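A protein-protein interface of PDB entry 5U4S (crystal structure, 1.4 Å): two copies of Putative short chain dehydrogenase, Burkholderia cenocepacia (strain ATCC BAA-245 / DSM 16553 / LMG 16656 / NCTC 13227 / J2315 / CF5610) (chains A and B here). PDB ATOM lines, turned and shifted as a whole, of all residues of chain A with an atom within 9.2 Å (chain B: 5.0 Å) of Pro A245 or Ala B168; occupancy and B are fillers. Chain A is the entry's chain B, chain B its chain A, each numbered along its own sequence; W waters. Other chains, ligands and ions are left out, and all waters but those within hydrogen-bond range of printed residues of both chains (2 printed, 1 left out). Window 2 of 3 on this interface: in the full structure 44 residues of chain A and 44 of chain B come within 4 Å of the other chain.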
ATOM      1  N   PRO A  95      30.940 -17.531  27.916  1.00  0.00           N
ATOM      2  CA  PRO A  95      29.830 -17.658  28.868  1.00  0.00           C
ATOM      3  C   PRO A  95      30.332 -17.549  30.300  1.00  0.00           C
ATOM      4  O   PRO A  95      31.530 -17.683  30.580  1.00  0.00           O
ATOM      5  CB  PRO A  95      29.279 -19.056  28.573  1.00  0.00           C
ATOM      6  CG  PRO A  95      30.450 -19.820  28.031  1.00  0.00           C
ATOM      7  CD  PRO A  95      31.264 -18.808  27.246  1.00  0.00           C
ATOM      8  N   VAL A  96      29.389 -17.315  31.224  1.00  0.00           N
ATOM      9  CA  VAL A  96      29.768 -17.190  32.638  1.00  0.00           C
ATOM     10  C   VAL A  96      30.136 -18.530  33.261  1.00  0.00           C
ATOM     11  O   VAL A  96      31.015 -18.584  34.125  1.00  0.00           O
ATOM     12  CB  VAL A  96      28.725 -16.426  33.477  1.00  0.00           C
ATOM     13  CG1 VAL A  96      28.817 -14.941  33.162  1.00  0.00           C
ATOM     14  CG2 VAL A  96      27.311 -16.965  33.253  1.00  0.00           C
ATOM     15  N   LEU A  97      29.448 -19.615  32.894  1.00  0.00           N
ATOM     16  CA  LEU A  97      29.740 -20.897  33.542  1.00  0.00           C
ATOM     17  C   LEU A  97      30.767 -21.708  32.759  1.00  0.00           C
ATOM     18  O   LEU A  97      31.856 -22.008  33.269  1.00  0.00           O
ATOM     19  CB  LEU A  97      28.460 -21.716  33.771  1.00  0.00           C
ATOM     20  CG  LEU A  97      27.367 -21.032  34.590  1.00  0.00           C
ATOM     21  CD1 LEU A  97      26.283 -22.032  34.932  1.00  0.00           C
ATOM     22  CD2 LEU A  97      27.930 -20.388  35.868  1.00  0.00           C
ATOM     23  N   GLU A  98      30.437 -22.080  31.527  1.00  0.00           N
ATOM     24  CA  GLU A  98      31.326 -22.932  30.738  1.00  0.00           C
ATOM     25  C   GLU A  98      32.420 -22.124  30.033  1.00  0.00           C
ATOM     26  O   GLU A  98      32.588 -22.238  28.817  1.00  0.00           O
ATOM     27  CB  GLU A  98      30.506 -23.716  29.716  1.00  0.00           C
ATOM     28  CG  GLU A  98      31.143 -25.041  29.311  1.00  0.00           C
ATOM     29  CD  GLU A  98      30.277 -25.839  28.348  1.00  0.00           C
ATOM     30  OE1 GLU A  98      30.815 -26.759  27.695  1.00  0.00           O
ATOM     31  OE2 GLU A  98      29.066 -25.548  28.244  1.00  0.00           O
ATOM     32  N   ALA A 145      21.667 -10.462  28.701  1.00  0.00           N
ATOM     33  CA  ALA A 145      22.804 -11.293  28.333  1.00  0.00           C
ATOM     34  C   ALA A 145      22.560 -12.012  27.015  1.00  0.00           C
ATOM     35  O   ALA A 145      21.447 -12.454  26.724  1.00  0.00           O
ATOM     36  CB  ALA A 145      23.050 -12.323  29.430  1.00  0.00           C
ATOM     37  N   LEU A 146      23.612 -12.097  26.198  1.00  0.00           N
ATOM     38  CA  LEU A 146      23.737 -13.150  25.210  1.00  0.00           C
ATOM     39  C   LEU A 146      24.545 -14.248  25.883  1.00  0.00           C
ATOM     40  O   LEU A 146      25.652 -13.967  26.370  1.00  0.00           O
ATOM     41  CB  LEU A 146      24.481 -12.629  23.986  1.00  0.00           C
ATOM     42  CG  LEU A 146      24.742 -13.521  22.784  1.00  0.00           C
ATOM     43  CD1 LEU A 146      23.410 -13.947  22.189  1.00  0.00           C
ATOM     44  CD2 LEU A 146      25.538 -12.703  21.754  1.00  0.00           C
ATOM     45  N   PRO A 147      24.022 -15.474  25.993  1.00  0.00           N
ATOM     46  CA  PRO A 147      24.702 -16.500  26.804  1.00  0.00           C
ATOM     47  C   PRO A 147      26.143 -16.740  26.406  1.00  0.00           C
ATOM     48  O   PRO A 147      26.993 -16.912  27.290  1.00  0.00           O
ATOM     49  CB  PRO A 147      23.802 -17.726  26.629  1.00  0.00           C
ATOM     50  CG  PRO A 147      22.424 -17.083  26.493  1.00  0.00           C
ATOM     51  CD  PRO A 147      22.670 -15.909  25.589  1.00  0.00           C
ATOM     52  N   SER A 148      26.457 -16.677  25.111  1.00  0.00           N
ATOM     53  CA  SER A 148      27.835 -16.924  24.695  1.00  0.00           C
ATOM     54  C   SER A 148      28.797 -15.818  25.092  1.00  0.00           C
ATOM     55  O   SER A 148      30.006 -16.032  24.988  1.00  0.00           O
ATOM     56  CB  SER A 148      27.906 -17.114  23.186  1.00  0.00           C
ATOM     57  OG  SER A 148      27.520 -15.920  22.534  1.00  0.00           O
ATOM     58  N   ALA A 150      28.137 -13.737  28.104  1.00  0.00           N
ATOM     59  CA  ALA A 150      27.397 -13.206  29.241  1.00  0.00           C
ATOM     60  C   ALA A 150      28.288 -12.417  30.193  1.00  0.00           C
ATOM     61  O   ALA A 150      27.797 -11.517  30.887  1.00  0.00           O
ATOM     62  CB  ALA A 150      26.631 -14.306  29.990  1.00  0.00           C
ATOM     63  N   HIS A 239      12.688 -12.450  27.229  1.00  0.00           N
ATOM     64  CA  HIS A 239      13.614 -13.285  27.985  1.00  0.00           C
ATOM     65  C   HIS A 239      13.429 -14.766  27.677  1.00  0.00           C
ATOM     66  O   HIS A 239      14.409 -15.493  27.478  1.00  0.00           O
ATOM     67  CB  HIS A 239      13.383 -13.061  29.466  1.00  0.00           C
ATOM     68  CG  HIS A 239      14.019 -11.827  29.997  1.00  0.00           C
ATOM     69  ND1 HIS A 239      13.665 -11.299  31.218  1.00  0.00           N
ATOM     70  CD2 HIS A 239      15.003 -11.036  29.507  1.00  0.00           C
ATOM     71  CE1 HIS A 239      14.407 -10.232  31.463  1.00  0.00           C
ATOM     72  NE2 HIS A 239      15.224 -10.051  30.439  1.00  0.00           N
ATOM     73  N   ALA A 240      12.180 -15.250  27.699  1.00  0.00           N
ATOM     74  CA  ALA A 240      11.963 -16.680  27.494  1.00  0.00           C
ATOM     75  C   ALA A 240      12.449 -17.108  26.121  1.00  0.00           C
ATOM     76  O   ALA A 240      12.999 -18.205  25.963  1.00  0.00           O
ATOM     77  CB  ALA A 240      10.486 -17.038  27.687  1.00  0.00           C
ATOM     78  N   ARG A 241      12.281 -16.240  25.125  1.00  0.00           N
ATOM     79  CA  ARG A 241      12.747 -16.549  23.779  1.00  0.00           C
ATOM     80  C   ARG A 241      14.274 -16.522  23.701  1.00  0.00           C
ATOM     81  O   ARG A 241      14.896 -17.470  23.200  1.00  0.00           O
ATOM     82  CB  ARG A 241      12.132 -15.554  22.795  1.00  0.00           C
ATOM     83  CG  ARG A 241      12.462 -15.834  21.352  1.00  0.00           C
ATOM     84  CD  ARG A 241      11.739 -14.876  20.415  1.00  0.00           C
ATOM     85  NE  ARG A 241      12.281 -13.521  20.464  1.00  0.00           N
ATOM     86  CZ  ARG A 241      13.418 -13.145  19.881  1.00  0.00           C
ATOM     87  NH1 ARG A 241      14.150 -14.029  19.213  1.00  0.00           N
ATOM     88  NH2 ARG A 241      13.829 -11.887  19.970  1.00  0.00           N
ATOM     89  N   LEU A 242      14.894 -15.451  24.212  1.00  0.00           N
ATOM     90  CA  LEU A 242      16.333 -15.243  24.052  1.00  0.00           C
ATOM     91  C   LEU A 242      17.187 -16.124  24.955  1.00  0.00           C
ATOM     92  O   LEU A 242      18.355 -16.355  24.632  1.00  0.00           O
ATOM     93  CB  LEU A 242      16.716 -13.792  24.345  1.00  0.00           C
ATOM     94  CG  LEU A 242      16.330 -12.690  23.359  1.00  0.00           C
ATOM     95  CD1 LEU A 242      16.810 -11.345  23.880  1.00  0.00           C
ATOM     96  CD2 LEU A 242      16.914 -12.971  21.996  1.00  0.00           C
ATOM     97  N   LEU A 243      16.659 -16.601  26.080  1.00  0.00           N
ATOM     98  CA  LEU A 243      17.483 -17.301  27.064  1.00  0.00           C
ATOM     99  C   LEU A 243      17.118 -18.769  27.238  1.00  0.00           C
ATOM    100  O   LEU A 243      17.562 -19.389  28.210  1.00  0.00           O
ATOM    101  CB  LEU A 243      17.441 -16.582  28.415  1.00  0.00           C
ATOM    102  CG  LEU A 243      17.862 -15.106  28.407  1.00  0.00           C
ATOM    103  CD1 LEU A 243      17.448 -14.378  29.708  1.00  0.00           C
ATOM    104  CD2 LEU A 243      19.366 -14.995  28.169  1.00  0.00           C
ATOM    105  N   THR A 244      16.328 -19.344  26.343  1.00  0.00           N
ATOM    106  CA  THR A 244      16.048 -20.779  26.382  1.00  0.00           C
ATOM    107  C   THR A 244      16.610 -21.428  25.125  1.00  0.00           C
ATOM    108  O   THR A 244      16.037 -21.254  24.032  1.00  0.00           O
ATOM    109  CB  THR A 244      14.545 -21.037  26.495  1.00  0.00           C
ATOM    110  OG1 THR A 244      13.863 -20.340  25.444  1.00  0.00           O
ATOM    111  CG2 THR A 244      14.013 -20.568  27.858  1.00  0.00           C
ATOM    112  N   PRO A 245      17.729 -22.168  25.213  1.00  0.00           N
ATOM    113  CA  PRO A 245      18.349 -22.853  24.071  1.00  0.00           C
ATOM    114  C   PRO A 245      17.481 -23.983  23.524  1.00  0.00           C
ATOM    115  O   PRO A 245      16.517 -24.413  24.161  1.00  0.00           O
ATOM    116  CB  PRO A 245      19.637 -23.437  24.665  1.00  0.00           C
ATOM    117  CG  PRO A 245      19.888 -22.646  25.899  1.00  0.00           C
ATOM    118  CD  PRO A 245      18.533 -22.312  26.437  1.00  0.00           C
ATOM    119  OXT PRO A 245      17.730 -24.493  22.430  1.00  0.00           O
ATOM    120  N   GLU B 164      21.170 -14.481  33.990  1.00  0.00           N
ATOM    121  CA  GLU B 164      20.547 -14.770  32.696  1.00  0.00           C
ATOM    122  C   GLU B 164      21.396 -15.725  31.870  1.00  0.00           C
ATOM    123  O   GLU B 164      20.877 -16.670  31.265  1.00  0.00           O
ATOM    124  CB  GLU B 164      20.327 -13.459  31.913  1.00  0.00           C
ATOM    125  CG  GLU B 164      19.296 -12.526  32.589  1.00  0.00           C
ATOM    126  CD  GLU B 164      19.340 -11.093  32.108  1.00  0.00           C
ATOM    127  OE1 GLU B 164      20.199 -10.737  31.266  1.00  0.00           O
ATOM    128  OE2 GLU B 164      18.460 -10.309  32.572  1.00  0.00           O
ATOM    129  N   GLY B 165      22.713 -15.475  31.806  1.00  0.00           N
ATOM    130  CA  GLY B 165      23.572 -16.379  31.060  1.00  0.00           C
ATOM    131  C   GLY B 165      23.578 -17.780  31.646  1.00  0.00           C
ATOM    132  O   GLY B 165      23.489 -18.771  30.916  1.00  0.00           O
ATOM    133  N   ALA B 166      23.687 -17.871  32.977  1.00  0.00           N
ATOM    134  CA  ALA B 166      23.675 -19.169  33.640  1.00  0.00           C
ATOM    135  C   ALA B 166      22.345 -19.883  33.423  1.00  0.00           C
ATOM    136  O   ALA B 166      22.320 -21.100  33.215  1.00  0.00           O
ATOM    137  CB  ALA B 166      23.949 -18.968  35.121  1.00  0.00           C
ATOM    138  N   ARG B 167      21.229 -19.138  33.465  1.00  0.00           N
ATOM    139  CA  ARG B 167      19.925 -19.739  33.198  1.00  0.00           C
ATOM    140  C   ARG B 167      19.915 -20.423  31.839  1.00  0.00           C
ATOM    141  O   ARG B 167      19.465 -21.568  31.707  1.00  0.00           O
ATOM    142  CB  ARG B 167      18.833 -18.669  33.289  1.00  0.00           C
ATOM    143  CG  ARG B 167      17.409 -19.179  33.007  1.00  0.00           C
ATOM    144  CD  ARG B 167      16.990 -18.821  31.605  1.00  0.00           C
ATOM    145  NE  ARG B 167      15.590 -19.150  31.367  1.00  0.00           N
ATOM    146  CZ  ARG B 167      14.596 -18.268  31.421  1.00  0.00           C
ATOM    147  NH1 ARG B 167      14.846 -16.995  31.689  1.00  0.00           N
ATOM    148  NH2 ARG B 167      13.346 -18.659  31.196  1.00  0.00           N
ATOM    149  N   ALA B 168      20.432 -19.750  30.808  1.00  0.00           N
ATOM    150  CA  ALA B 168      20.458 -20.359  29.486  1.00  0.00           C
ATOM    151  C   ALA B 168      21.379 -21.576  29.442  1.00  0.00           C
ATOM    152  O   ALA B 168      21.056 -22.577  28.800  1.00  0.00           O
ATOM    153  CB  ALA B 168      20.893 -19.325  28.451  1.00  0.00           C
ATOM    154  N   GLU B 169      22.538 -21.504  30.107  1.00  0.00           N
ATOM    155  CA  GLU B 169      23.470 -22.626  30.055  1.00  0.00           C
ATOM    156  C   GLU B 169      22.922 -23.855  30.776  1.00  0.00           C
ATOM    157  O   GLU B 169      23.218 -24.989  30.375  1.00  0.00           O
ATOM    158  CB  GLU B 169      24.799 -22.232  30.710  1.00  0.00           C
ATOM    159  CG  GLU B 169      25.610 -21.164  29.952  1.00  0.00           C
ATOM    160  CD  GLU B 169      26.979 -20.946  30.568  1.00  0.00           C
ATOM    161  OE1 GLU B 169      27.840 -21.849  30.374  1.00  0.00           O
ATOM    162  OE2 GLU B 169      27.179 -19.926  31.250  1.00  0.00           O
ATOM    163  N   LEU B 170      22.152 -23.647  31.852  1.00  0.00           N
ATOM    164  CA  LEU B 170      21.701 -24.738  32.707  1.00  0.00           C
ATOM    165  C   LEU B 170      20.331 -25.279  32.323  1.00  0.00           C
ATOM    166  O   LEU B 170      19.998 -26.404  32.716  1.00  0.00           O
ATOM    167  CB  LEU B 170      21.694 -24.291  34.171  1.00  0.00           C
ATOM    168  CG  LEU B 170      23.093 -24.105  34.772  1.00  0.00           C
ATOM    169  CD1 LEU B 170      23.011 -23.482  36.138  1.00  0.00           C
ATOM    170  CD2 LEU B 170      23.765 -25.479  34.881  1.00  0.00           C
ATOM    171  N   ALA B 171      19.529 -24.515  31.583  1.00  0.00           N
ATOM    172  CA  ALA B 171      18.179 -24.954  31.236  1.00  0.00           C
ATOM    173  C   ALA B 171      18.120 -26.327  30.572  1.00  0.00           C
ATOM    174  O   ALA B 171      17.209 -27.102  30.910  1.00  0.00           O
ATOM    175  CB  ALA B 171      17.488 -23.892  30.367  1.00  0.00           C
ATOM    176  N   PRO B 172      19.007 -26.696  29.639  1.00  0.00           N
ATOM    177  CA  PRO B 172      18.940 -28.043  29.050  1.00  0.00           C
ATOM    178  C   PRO B 172      19.401 -29.146  29.985  1.00  0.00           C
ATOM    179  O   PRO B 172      19.305 -30.324  29.613  1.00  0.00           O
ATOM    180  CB  PRO B 172      19.886 -27.940  27.841  1.00  0.00           C
ATOM    181  CG  PRO B 172      20.148 -26.485  27.650  1.00  0.00           C
ATOM    182  CD  PRO B 172      20.062 -25.890  29.000  1.00  0.00           C
HETATM  183  O   HOH W   1      27.304 -23.752  28.574  1.00  0.00           O
HETATM  184  O   HOH W   2      17.393  -8.667  30.697  1.00  0.00           O
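The side-chain carboxylate (OE2) of Glu B169 sits at hydrogen-bond distance from the backbone NH (N) of Leu A97 (2.8 Å). The side-chain carboxylate (OE1) of Glu B164 is in hydrogen-bond range of the backbone NH (N) of Ala A145, at 3.0 Å. OE2 of Glu B169 lies within hydrogen-bond range of N of Val A96 (3.4 Å). OE1 of Glu B169 sits at hydrogen-bond distance from N of Glu A98 (2.9 Å).
Of the 16 printed residues of chain A, 11 touch a printed residue of chain B. Printed residues of chain A that touch a printed residue of chain B: Pro A95, Val A96, Leu A97, Glu A98, Ala A145, Pro A147, Ala A150, His A239, Leu A243, Thr A244 and Pro A245. Hydrophobic or aromatic side chains of chain A that line the printed part of chain B: Pro A95, Val A96, Leu A97, Ala A145, Pro A147, Ala A150, His A239, Leu A243 and Pro A245. Of the 9 printed residues of chain B, 7 touch a printed residue of chain A. Hydrophobic or aromatic side chains of chain B within 4 Å of the printed part of chain A: Ala B166, Ala B168 and Leu B170. Among the printed residues, 17 pairs touch across the chains.
Glu B169 touches Pro A95 (OE2 to CB, 3.5 Å). CG2 of Val A96 touches N of Ala B166, 3.7 Å away. Leu B170 touches Leu A97. CB of Ala A145 touches N of Gly B165 (3.96 Å). CG of Pro A147 touches CB of Ala B168, 3.3 Å away. Ala A150 touches Gly B165 (CB to CA, 3.8 Å). Glu B164 touches His A239 (OE2 to NE2, 3.9 Å). CD1 of Leu A243 touches CB of Glu B164, 3.7 Å away. O of Leu A243 touches CD of Arg B167, 3.5 Å away. Pro A245 touches Ala B168.
Water W1 lies within hydrogen-bond range of the side-chain carboxylate of Glu A98 (2.5 Å) and the side-chain carboxylate of Glu B169 (2.7 Å). Water W2 lies within hydrogen-bond range of NE2 of His A239 (2.6 Å) and OE2 of Glu B164 (2.7 Å).
Printed residues of chain B within 4 Å of Pro A95: Glu B169. Printed residues of chain B within 4 Å of Leu A97: Ala B166 (3.9 Å), Glu B169 (2.8 Å) and Leu B170 (3.8 Å). Of the printed residues of chain B, Pro A245 touches Ala B168. Gly B165 touches two residues of chain A. Of the printed residues of chain A, Ala B168 touches Pro A147, Leu A243 and Pro A245. Ala B171 touches none of the printed residues of chain A.
No position is printed for both chains. Of the 17 pairs that touch across the chains among the printed residues, none has its exchanged pair printed and touching as well.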
